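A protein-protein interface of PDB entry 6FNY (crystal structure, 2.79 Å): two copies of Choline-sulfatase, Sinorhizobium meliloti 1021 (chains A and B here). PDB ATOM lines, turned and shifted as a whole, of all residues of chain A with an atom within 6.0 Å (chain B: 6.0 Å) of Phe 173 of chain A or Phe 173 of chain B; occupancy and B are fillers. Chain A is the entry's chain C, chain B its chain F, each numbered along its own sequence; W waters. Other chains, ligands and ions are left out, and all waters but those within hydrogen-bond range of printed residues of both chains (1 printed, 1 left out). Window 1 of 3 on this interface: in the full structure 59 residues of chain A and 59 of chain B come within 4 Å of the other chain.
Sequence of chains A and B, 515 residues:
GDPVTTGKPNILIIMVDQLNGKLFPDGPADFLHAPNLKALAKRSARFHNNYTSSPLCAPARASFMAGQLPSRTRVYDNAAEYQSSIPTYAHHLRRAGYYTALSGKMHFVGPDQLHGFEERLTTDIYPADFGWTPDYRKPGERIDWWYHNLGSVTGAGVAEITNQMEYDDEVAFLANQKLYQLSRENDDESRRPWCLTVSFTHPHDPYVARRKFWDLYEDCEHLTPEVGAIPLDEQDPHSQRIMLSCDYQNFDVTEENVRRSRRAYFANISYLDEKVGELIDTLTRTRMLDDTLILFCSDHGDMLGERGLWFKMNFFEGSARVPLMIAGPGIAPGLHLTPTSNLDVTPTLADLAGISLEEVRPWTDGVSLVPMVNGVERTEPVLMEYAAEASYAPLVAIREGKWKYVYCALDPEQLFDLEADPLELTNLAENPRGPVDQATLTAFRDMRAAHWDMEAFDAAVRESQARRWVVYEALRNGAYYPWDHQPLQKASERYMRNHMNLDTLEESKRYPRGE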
ATOM      1  N   GLU A 166      10.645 -19.453  -6.265  1.00  0.00           N
ATOM      2  CA  GLU A 166      10.328 -20.557  -5.368  1.00  0.00           C
ATOM      3  C   GLU A 166       8.845 -20.562  -5.025  1.00  0.00           C
ATOM      4  O   GLU A 166       8.203 -21.619  -5.016  1.00  0.00           O
ATOM      5  CB  GLU A 166      11.173 -20.466  -4.097  1.00  0.00           C
ATOM      6  CG  GLU A 166      10.479 -20.992  -2.849  1.00  0.00           C
ATOM      7  CD  GLU A 166      11.408 -21.097  -1.655  1.00  0.00           C
ATOM      8  OE1 GLU A 166      11.237 -22.038  -0.852  1.00  0.00           O
ATOM      9  OE2 GLU A 166      12.303 -20.236  -1.517  1.00  0.00           O
ATOM     10  N   ASP A 168       6.178 -19.158  -6.736  1.00  0.00           N
ATOM     11  CA  ASP A 168       5.323 -19.479  -7.873  1.00  0.00           C
ATOM     12  C   ASP A 168       5.511 -20.916  -8.338  1.00  0.00           C
ATOM     13  O   ASP A 168       4.560 -21.529  -8.839  1.00  0.00           O
ATOM     14  CB  ASP A 168       5.595 -18.512  -9.023  1.00  0.00           C
ATOM     15  CG  ASP A 168       4.941 -17.166  -8.812  1.00  0.00           C
ATOM     16  OD1 ASP A 168       4.065 -17.063  -7.926  1.00  0.00           O
ATOM     17  OD2 ASP A 168       5.305 -16.210  -9.531  1.00  0.00           O
ATOM     18  N   ASP A 169       6.717 -21.469  -8.186  1.00  0.00           N
ATOM     19  CA  ASP A 169       6.944 -22.849  -8.601  1.00  0.00           C
ATOM     20  C   ASP A 169       6.083 -23.814  -7.795  1.00  0.00           C
ATOM     21  O   ASP A 169       5.553 -24.787  -8.343  1.00  0.00           O
ATOM     22  CB  ASP A 169       8.426 -23.210  -8.475  1.00  0.00           C
ATOM     23  CG  ASP A 169       9.237 -22.794  -9.695  1.00  0.00           C
ATOM     24  OD1 ASP A 169       8.635 -22.586 -10.769  1.00  0.00           O
ATOM     25  OD2 ASP A 169      10.478 -22.682  -9.587  1.00  0.00           O
ATOM     26  N   GLU A 170       5.917 -23.558  -6.494  1.00  0.00           N
ATOM     27  CA  GLU A 170       5.070 -24.424  -5.683  1.00  0.00           C
ATOM     28  C   GLU A 170       3.613 -23.987  -5.677  1.00  0.00           C
ATOM     29  O   GLU A 170       2.740 -24.797  -5.344  1.00  0.00           O
ATOM     30  CB  GLU A 170       5.607 -24.523  -4.248  1.00  0.00           C
ATOM     31  CG  GLU A 170       5.203 -23.429  -3.284  1.00  0.00           C
ATOM     32  CD  GLU A 170       5.511 -23.809  -1.839  1.00  0.00           C
ATOM     33  OE1 GLU A 170       5.837 -24.991  -1.589  1.00  0.00           O
ATOM     34  OE2 GLU A 170       5.439 -22.926  -0.958  1.00  0.00           O
ATOM     35  N   VAL A 171       3.329 -22.741  -6.052  1.00  0.00           N
ATOM     36  CA  VAL A 171       1.948 -22.365  -6.327  1.00  0.00           C
ATOM     37  C   VAL A 171       1.435 -23.119  -7.545  1.00  0.00           C
ATOM     38  O   VAL A 171       0.315 -23.645  -7.545  1.00  0.00           O
ATOM     39  CB  VAL A 171       1.838 -20.842  -6.515  1.00  0.00           C
ATOM     40  CG1 VAL A 171       0.503 -20.477  -7.146  1.00  0.00           C
ATOM     41  CG2 VAL A 171       2.016 -20.130  -5.184  1.00  0.00           C
ATOM     42  N   ALA A 172       2.254 -23.201  -8.595  1.00  0.00           N
ATOM     43  CA  ALA A 172       1.836 -23.870  -9.820  1.00  0.00           C
ATOM     44  C   ALA A 172       1.687 -25.370  -9.606  1.00  0.00           C
ATOM     45  O   ALA A 172       0.674 -25.963  -9.996  1.00  0.00           O
ATOM     46  CB  ALA A 172       2.838 -23.583 -10.938  1.00  0.00           C
ATOM     47  N   PHE A 173       2.691 -26.001  -8.991  1.00  0.00           N
ATOM     48  CA  PHE A 173       2.658 -27.450  -8.822  1.00  0.00           C
ATOM     49  C   PHE A 173       1.464 -27.880  -7.984  1.00  0.00           C
ATOM     50  O   PHE A 173       0.726 -28.800  -8.360  1.00  0.00           O
ATOM     51  CB  PHE A 173       3.952 -27.946  -8.180  1.00  0.00           C
ATOM     52  CG  PHE A 173       3.870 -29.365  -7.706  1.00  0.00           C
ATOM     53  CD1 PHE A 173       4.000 -30.411  -8.599  1.00  0.00           C
ATOM     54  CD2 PHE A 173       3.629 -29.654  -6.372  1.00  0.00           C
ATOM     55  CE1 PHE A 173       3.910 -31.716  -8.173  1.00  0.00           C
ATOM     56  CE2 PHE A 173       3.536 -30.959  -5.942  1.00  0.00           C
ATOM     57  CZ  PHE A 173       3.674 -31.988  -6.846  1.00  0.00           C
ATOM     58  N   LEU A 174       1.269 -27.235  -6.831  1.00  0.00           N
ATOM     59  CA  LEU A 174       0.159 -27.605  -5.960  1.00  0.00           C
ATOM     60  C   LEU A 174      -1.181 -27.369  -6.639  1.00  0.00           C
ATOM     61  O   LEU A 174      -2.143 -28.104  -6.387  1.00  0.00           O
ATOM     62  CB  LEU A 174       0.249 -26.831  -4.643  1.00  0.00           C
ATOM     63  CG  LEU A 174       1.371 -27.307  -3.713  1.00  0.00           C
ATOM     64  CD1 LEU A 174       1.644 -26.310  -2.596  1.00  0.00           C
ATOM     65  CD2 LEU A 174       1.042 -28.676  -3.143  1.00  0.00           C
ATOM     66  N   ALA A 175      -1.258 -26.365  -7.516  1.00  0.00           N
ATOM     67  CA  ALA A 175      -2.486 -26.135  -8.267  1.00  0.00           C
ATOM     68  C   ALA A 175      -2.752 -27.272  -9.247  1.00  0.00           C
ATOM     69  O   ALA A 175      -3.885 -27.756  -9.352  1.00  0.00           O
ATOM     70  CB  ALA A 175      -2.409 -24.796  -9.000  1.00  0.00           C
ATOM     71  N   ASN A 176      -1.717 -27.716  -9.966  1.00  0.00           N
ATOM     72  CA  ASN A 176      -1.890 -28.830 -10.892  1.00  0.00           C
ATOM     73  C   ASN A 176      -2.132 -30.143 -10.157  1.00  0.00           C
ATOM     74  O   ASN A 176      -2.865 -31.005 -10.656  1.00  0.00           O
ATOM     75  CB  ASN A 176      -0.670 -28.946 -11.804  1.00  0.00           C
ATOM     76  CG  ASN A 176      -0.661 -27.894 -12.891  1.00  0.00           C
ATOM     77  OD1 ASN A 176      -1.398 -27.994 -13.872  1.00  0.00           O
ATOM     78  ND2 ASN A 176       0.178 -26.876 -12.726  1.00  0.00           N
ATOM     79  N   GLN A 177      -1.529 -30.315  -8.978  1.00  0.00           N
ATOM     80  CA  GLN A 177      -1.807 -31.500  -8.175  1.00  0.00           C
ATOM     81  C   GLN A 177      -3.257 -31.515  -7.705  1.00  0.00           C
ATOM     82  O   GLN A 177      -3.892 -32.576  -7.652  1.00  0.00           O
ATOM     83  CB  GLN A 177      -0.846 -31.560  -6.986  1.00  0.00           C
ATOM     84  CG  GLN A 177      -1.388 -32.282  -5.762  1.00  0.00           C
ATOM     85  CD  GLN A 177      -0.348 -32.436  -4.670  1.00  0.00           C
ATOM     86  OE1 GLN A 177      -0.474 -31.859  -3.590  1.00  0.00           O
ATOM     87  NE2 GLN A 177       0.688 -33.218  -4.948  1.00  0.00           N
ATOM     88  N   LYS A 178      -3.801 -30.342  -7.371  1.00  0.00           N
ATOM     89  CA  LYS A 178      -5.196 -30.270  -6.951  1.00  0.00           C
ATOM     90  C   LYS A 178      -6.138 -30.608  -8.100  1.00  0.00           C
ATOM     91  O   LYS A 178      -7.162 -31.270  -7.894  1.00  0.00           O
ATOM     92  CB  LYS A 178      -5.509 -28.881  -6.394  1.00  0.00           C
ATOM     93  CG  LYS A 178      -6.661 -28.865  -5.404  1.00  0.00           C
ATOM     94  CD  LYS A 178      -6.331 -29.695  -4.175  1.00  0.00           C
ATOM     95  CE  LYS A 178      -7.589 -30.127  -3.450  1.00  0.00           C
ATOM     96  NZ  LYS A 178      -7.297 -31.088  -2.353  1.00  0.00           N
ATOM     97  N   GLU A 278       0.735 -25.358 -18.433  1.00  0.00           N
ATOM     98  CA  GLU A 278       0.665 -26.541 -17.582  1.00  0.00           C
ATOM     99  C   GLU A 278      -0.747 -26.740 -17.047  1.00  0.00           C
ATOM    100  O   GLU A 278      -1.281 -27.854 -17.066  1.00  0.00           O
ATOM    101  CB  GLU A 278       1.664 -26.420 -16.433  1.00  0.00           C
ATOM    102  CG  GLU A 278       3.118 -26.552 -16.843  1.00  0.00           C
ATOM    103  CD  GLU A 278       4.063 -25.984 -15.802  1.00  0.00           C
ATOM    104  OE1 GLU A 278       5.234 -25.713 -16.142  1.00  0.00           O
ATOM    105  OE2 GLU A 278       3.629 -25.799 -14.644  1.00  0.00           O
ATOM    106  N   GLU B 166       0.782 -39.183  -8.481  1.00  0.00           N
ATOM    107  CA  GLU B 166       0.627 -38.078  -7.540  1.00  0.00           C
ATOM    108  C   GLU B 166       1.783 -38.050  -6.553  1.00  0.00           C
ATOM    109  O   GLU B 166       2.293 -36.978  -6.207  1.00  0.00           O
ATOM    110  CB  GLU B 166      -0.705 -38.190  -6.795  1.00  0.00           C
ATOM    111  CG  GLU B 166      -0.882 -37.144  -5.695  1.00  0.00           C
ATOM    112  CD  GLU B 166      -2.046 -37.442  -4.764  1.00  0.00           C
ATOM    113  OE1 GLU B 166      -2.175 -36.749  -3.732  1.00  0.00           O
ATOM    114  OE2 GLU B 166      -2.833 -38.365  -5.063  1.00  0.00           O
ATOM    115  N   ASP B 168       4.956 -39.420  -7.022  1.00  0.00           N
ATOM    116  CA  ASP B 168       6.239 -39.134  -7.653  1.00  0.00           C
ATOM    117  C   ASP B 168       6.305 -37.711  -8.190  1.00  0.00           C
ATOM    118  O   ASP B 168       7.389 -37.118  -8.228  1.00  0.00           O
ATOM    119  CB  ASP B 168       6.513 -40.137  -8.772  1.00  0.00           C
ATOM    120  CG  ASP B 168       7.101 -41.436  -8.257  1.00  0.00           C
ATOM    121  OD1 ASP B 168       7.577 -41.458  -7.100  1.00  0.00           O
ATOM    122  OD2 ASP B 168       7.091 -42.434  -9.008  1.00  0.00           O
ATOM    123  N   ASP B 169       5.170 -37.149  -8.617  1.00  0.00           N
ATOM    124  CA  ASP B 169       5.153 -35.738  -8.987  1.00  0.00           C
ATOM    125  C   ASP B 169       5.492 -34.864  -7.789  1.00  0.00           C
ATOM    126  O   ASP B 169       6.212 -33.867  -7.920  1.00  0.00           O
ATOM    127  CB  ASP B 169       3.788 -35.356  -9.558  1.00  0.00           C
ATOM    128  CG  ASP B 169       3.570 -35.891 -10.957  1.00  0.00           C
ATOM    129  OD1 ASP B 169       4.543 -36.395 -11.559  1.00  0.00           O
ATOM    130  OD2 ASP B 169       2.427 -35.810 -11.453  1.00  0.00           O
ATOM    131  N   GLU B 170       4.987 -35.230  -6.610  1.00  0.00           N
ATOM    132  CA  GLU B 170       5.330 -34.507  -5.391  1.00  0.00           C
ATOM    133  C   GLU B 170       6.793 -34.714  -5.025  1.00  0.00           C
ATOM    134  O   GLU B 170       7.500 -33.758  -4.687  1.00  0.00           O
ATOM    135  CB  GLU B 170       4.421 -34.953  -4.249  1.00  0.00           C
ATOM    136  CG  GLU B 170       4.353 -33.976  -3.097  1.00  0.00           C
ATOM    137  CD  GLU B 170       3.405 -34.438  -2.016  1.00  0.00           C
ATOM    138  OE1 GLU B 170       2.484 -33.668  -1.665  1.00  0.00           O
ATOM    139  OE2 GLU B 170       3.578 -35.572  -1.519  1.00  0.00           O
ATOM    140  N   VAL B 171       7.264 -35.962  -5.089  1.00  0.00           N
ATOM    141  CA  VAL B 171       8.649 -36.263  -4.743  1.00  0.00           C
ATOM    142  C   VAL B 171       9.602 -35.523  -5.669  1.00  0.00           C
ATOM    143  O   VAL B 171      10.604 -34.948  -5.228  1.00  0.00           O
ATOM    144  CB  VAL B 171       8.889 -37.784  -4.787  1.00  0.00           C
ATOM    145  CG1 VAL B 171      10.369 -38.097  -4.618  1.00  0.00           C
ATOM    146  CG2 VAL B 171       8.054 -38.481  -3.723  1.00  0.00           C
ATOM    147  N   ALA B 172       9.298 -35.516  -6.969  1.00  0.00           N
ATOM    148  CA  ALA B 172      10.185 -34.878  -7.935  1.00  0.00           C
ATOM    149  C   ALA B 172      10.214 -33.368  -7.751  1.00  0.00           C
ATOM    150  O   ALA B 172      11.274 -32.744  -7.871  1.00  0.00           O
ATOM    151  CB  ALA B 172       9.755 -35.237  -9.356  1.00  0.00           C
ATOM    152  N   PHE B 173       9.063 -32.758  -7.461  1.00  0.00           N
ATOM    153  CA  PHE B 173       9.039 -31.310  -7.301  1.00  0.00           C
ATOM    154  C   PHE B 173       9.772 -30.882  -6.035  1.00  0.00           C
ATOM    155  O   PHE B 173      10.616 -29.978  -6.071  1.00  0.00           O
ATOM    156  CB  PHE B 173       7.607 -30.785  -7.278  1.00  0.00           C
ATOM    157  CG  PHE B 173       7.524 -29.356  -6.851  1.00  0.00           C
ATOM    158  CD1 PHE B 173       7.941 -28.349  -7.706  1.00  0.00           C
ATOM    159  CD2 PHE B 173       7.089 -29.017  -5.580  1.00  0.00           C
ATOM    160  CE1 PHE B 173       7.898 -27.032  -7.317  1.00  0.00           C
ATOM    161  CE2 PHE B 173       7.045 -27.699  -5.185  1.00  0.00           C
ATOM    162  CZ  PHE B 173       7.456 -26.708  -6.058  1.00  0.00           C
ATOM    163  N   LEU B 174       9.453 -31.514  -4.901  1.00  0.00           N
ATOM    164  CA  LEU B 174      10.068 -31.120  -3.637  1.00  0.00           C
ATOM    165  C   LEU B 174      11.570 -31.371  -3.636  1.00  0.00           C
ATOM    166  O   LEU B 174      12.316 -30.658  -2.957  1.00  0.00           O
ATOM    167  CB  LEU B 174       9.399 -31.857  -2.477  1.00  0.00           C
ATOM    168  CG  LEU B 174       8.008 -31.336  -2.105  1.00  0.00           C
ATOM    169  CD1 LEU B 174       7.469 -32.039  -0.872  1.00  0.00           C
ATOM    170  CD2 LEU B 174       8.032 -29.828  -1.898  1.00  0.00           C
ATOM    171  N   ALA B 175      12.035 -32.371  -4.388  1.00  0.00           N
ATOM    172  CA  ALA B 175      13.472 -32.584  -4.515  1.00  0.00           C
ATOM    173  C   ALA B 175      14.129 -31.450  -5.294  1.00  0.00           C
ATOM    174  O   ALA B 175      15.205 -30.972  -4.917  1.00  0.00           O
ATOM    175  CB  ALA B 175      13.750 -33.929  -5.184  1.00  0.00           C
ATOM    176  N   ASN B 176      13.495 -31.005  -6.383  1.00  0.00           N
ATOM    177  CA  ASN B 176      14.034 -29.880  -7.138  1.00  0.00           C
ATOM    178  C   ASN B 176      13.912 -28.576  -6.360  1.00  0.00           C
ATOM    179  O   ASN B 176      14.747 -27.680  -6.522  1.00  0.00           O
ATOM    180  CB  ASN B 176      13.328 -29.764  -8.489  1.00  0.00           C
ATOM    181  CG  ASN B 176      13.809 -30.798  -9.489  1.00  0.00           C
ATOM    182  OD1 ASN B 176      14.976 -30.801  -9.885  1.00  0.00           O
ATOM    183  ND2 ASN B 176      12.911 -31.682  -9.905  1.00  0.00           N
ATOM    184  N   GLN B 177      12.885 -28.450  -5.514  1.00  0.00           N
ATOM    185  CA  GLN B 177      12.778 -27.273  -4.659  1.00  0.00           C
ATOM    186  C   GLN B 177      13.909 -27.233  -3.641  1.00  0.00           C
ATOM    187  O   GLN B 177      14.451 -26.161  -3.348  1.00  0.00           O
ATOM    188  CB  GLN B 177      11.421 -27.251  -3.953  1.00  0.00           C
ATOM    189  CG  GLN B 177      11.298 -26.172  -2.883  1.00  0.00           C
ATOM    190  CD  GLN B 177       9.894 -26.063  -2.311  1.00  0.00           C
ATOM    191  OE1 GLN B 177       9.493 -26.859  -1.462  1.00  0.00           O
ATOM    192  NE2 GLN B 177       9.143 -25.066  -2.767  1.00  0.00           N
ATOM    193  N   LYS B 178      14.282 -28.394  -3.097  1.00  0.00           N
ATOM    194  CA  LYS B 178      15.368 -28.437  -2.123  1.00  0.00           C
ATOM    195  C   LYS B 178      16.711 -28.156  -2.782  1.00  0.00           C
ATOM    196  O   LYS B 178      17.579 -27.514  -2.178  1.00  0.00           O
ATOM    197  CB  LYS B 178      15.389 -29.790  -1.412  1.00  0.00           C
ATOM    198  CG  LYS B 178      16.407 -29.872  -0.279  1.00  0.00           C
ATOM    199  CD  LYS B 178      15.723 -30.153   1.049  1.00  0.00           C
ATOM    200  CE  LYS B 178      15.250 -28.867   1.714  1.00  0.00           C
ATOM    201  NZ  LYS B 178      14.447 -29.145   2.937  1.00  0.00           N
ATOM    202  N   GLU B 278      15.110 -33.489 -14.987  1.00  0.00           N
ATOM    203  CA  GLU B 278      14.815 -32.290 -14.210  1.00  0.00           C
ATOM    204  C   GLU B 278      15.881 -32.054 -13.147  1.00  0.00           C
ATOM    205  O   GLU B 278      16.377 -30.933 -12.985  1.00  0.00           O
ATOM    206  CB  GLU B 278      13.432 -32.406 -13.568  1.00  0.00           C
ATOM    207  CG  GLU B 278      12.280 -32.216 -14.537  1.00  0.00           C
ATOM    208  CD  GLU B 278      10.990 -32.832 -14.035  1.00  0.00           C
ATOM    209  OE1 GLU B 278      10.953 -33.262 -12.863  1.00  0.00           O
ATOM    210  OE2 GLU B 278      10.014 -32.885 -14.813  1.00  0.00           O
HETATM  211  O   HOH W   1       9.108 -23.878  -5.015  1.00  0.00           O
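Among the printed residues, pairs that only touch across the chains: Phe 173 of chain A with Asp 169 of chain B (3.2 Å), Glu 170 of chain A with Phe 173 of chain B (3.3 Å), Phe 173 of chain A with Glu 170 of chain B (3.3 Å), Asp 169 of chain A with Phe 173 of chain B (3.4 Å), Glu 170 of chain A with Gln 177 of chain B (3.5 Å), Phe 173 of chain A with Phe 173 of chain B (3.6 Å) and Gln 177 of chain A with Glu 170 of chain B (3.8 Å).
Of chain B, only Asp 169, Glu 170 and Phe 173 come within 4 Å of Phe 173 of chain A. Printed residues of chain A within 4 Å of Glu 170 of chain B: Phe 173 and Gln 177. Of the printed residues of chain B, Gln 177 of chain A touches Glu 170. Of the printed residues of chain A, Gln 177 of chain B touches Glu 170 (3.5 Å). Of the printed residues of chain A, Asp 169 of chain B touches Phe 173. Asn 176 of chain A touches none of the printed residues of chain B. Glu 278 of chain B touches none of the printed residues of chain A. The nearest residue of chain B that does not touch Phe 173 of chain A is Glu 166 of chain B (5.2 Å). The nearest printed residue of chain A that does not touch Glu 170 of chain B is Leu 174 of chain A (5.4 Å).
Of the 13 printed residues of chain B, 4 touch a printed residue of chain A. Hydrophobic or aromatic side chains of chain B within 4 Å of the printed part of chain A: Phe 173. Of the 13 printed residues of chain A, 4 touch a printed residue of chain B. Hydrophobic or aromatic side chains of chain A that line the printed part of chain B: Phe 173. Among the printed residues, 7 pairs touch across the chains. Among the printed residues, no Asp or Glu carboxylate lies within 4 Å of a Lys or Arg side-chain nitrogen of the other chain.
Asp 169 of chain A touches Phe 173 of chain B, and with the chains exchanged Phe 173 of chain A touches Asp 169 of chain B. Glu 170 of chain A touches Phe 173 of chain B, and with the chains exchanged Phe 173 of chain A touches Glu 170 of chain B. Glu 170 of chain A touches Gln 177 of chain B, and with the chains exchanged Gln 177 of chain A touches Glu 170 of chain B. Phe 173 of chain B touches its own counterpart, Phe 173 of chain A. Of the 7 pairs that touch across the chains among the printed residues, 7 have their exchanged pair printed and touching as well.
Water W1 bridges O of Glu 166 of chain A and NE2 of Gln 177 of chain B.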
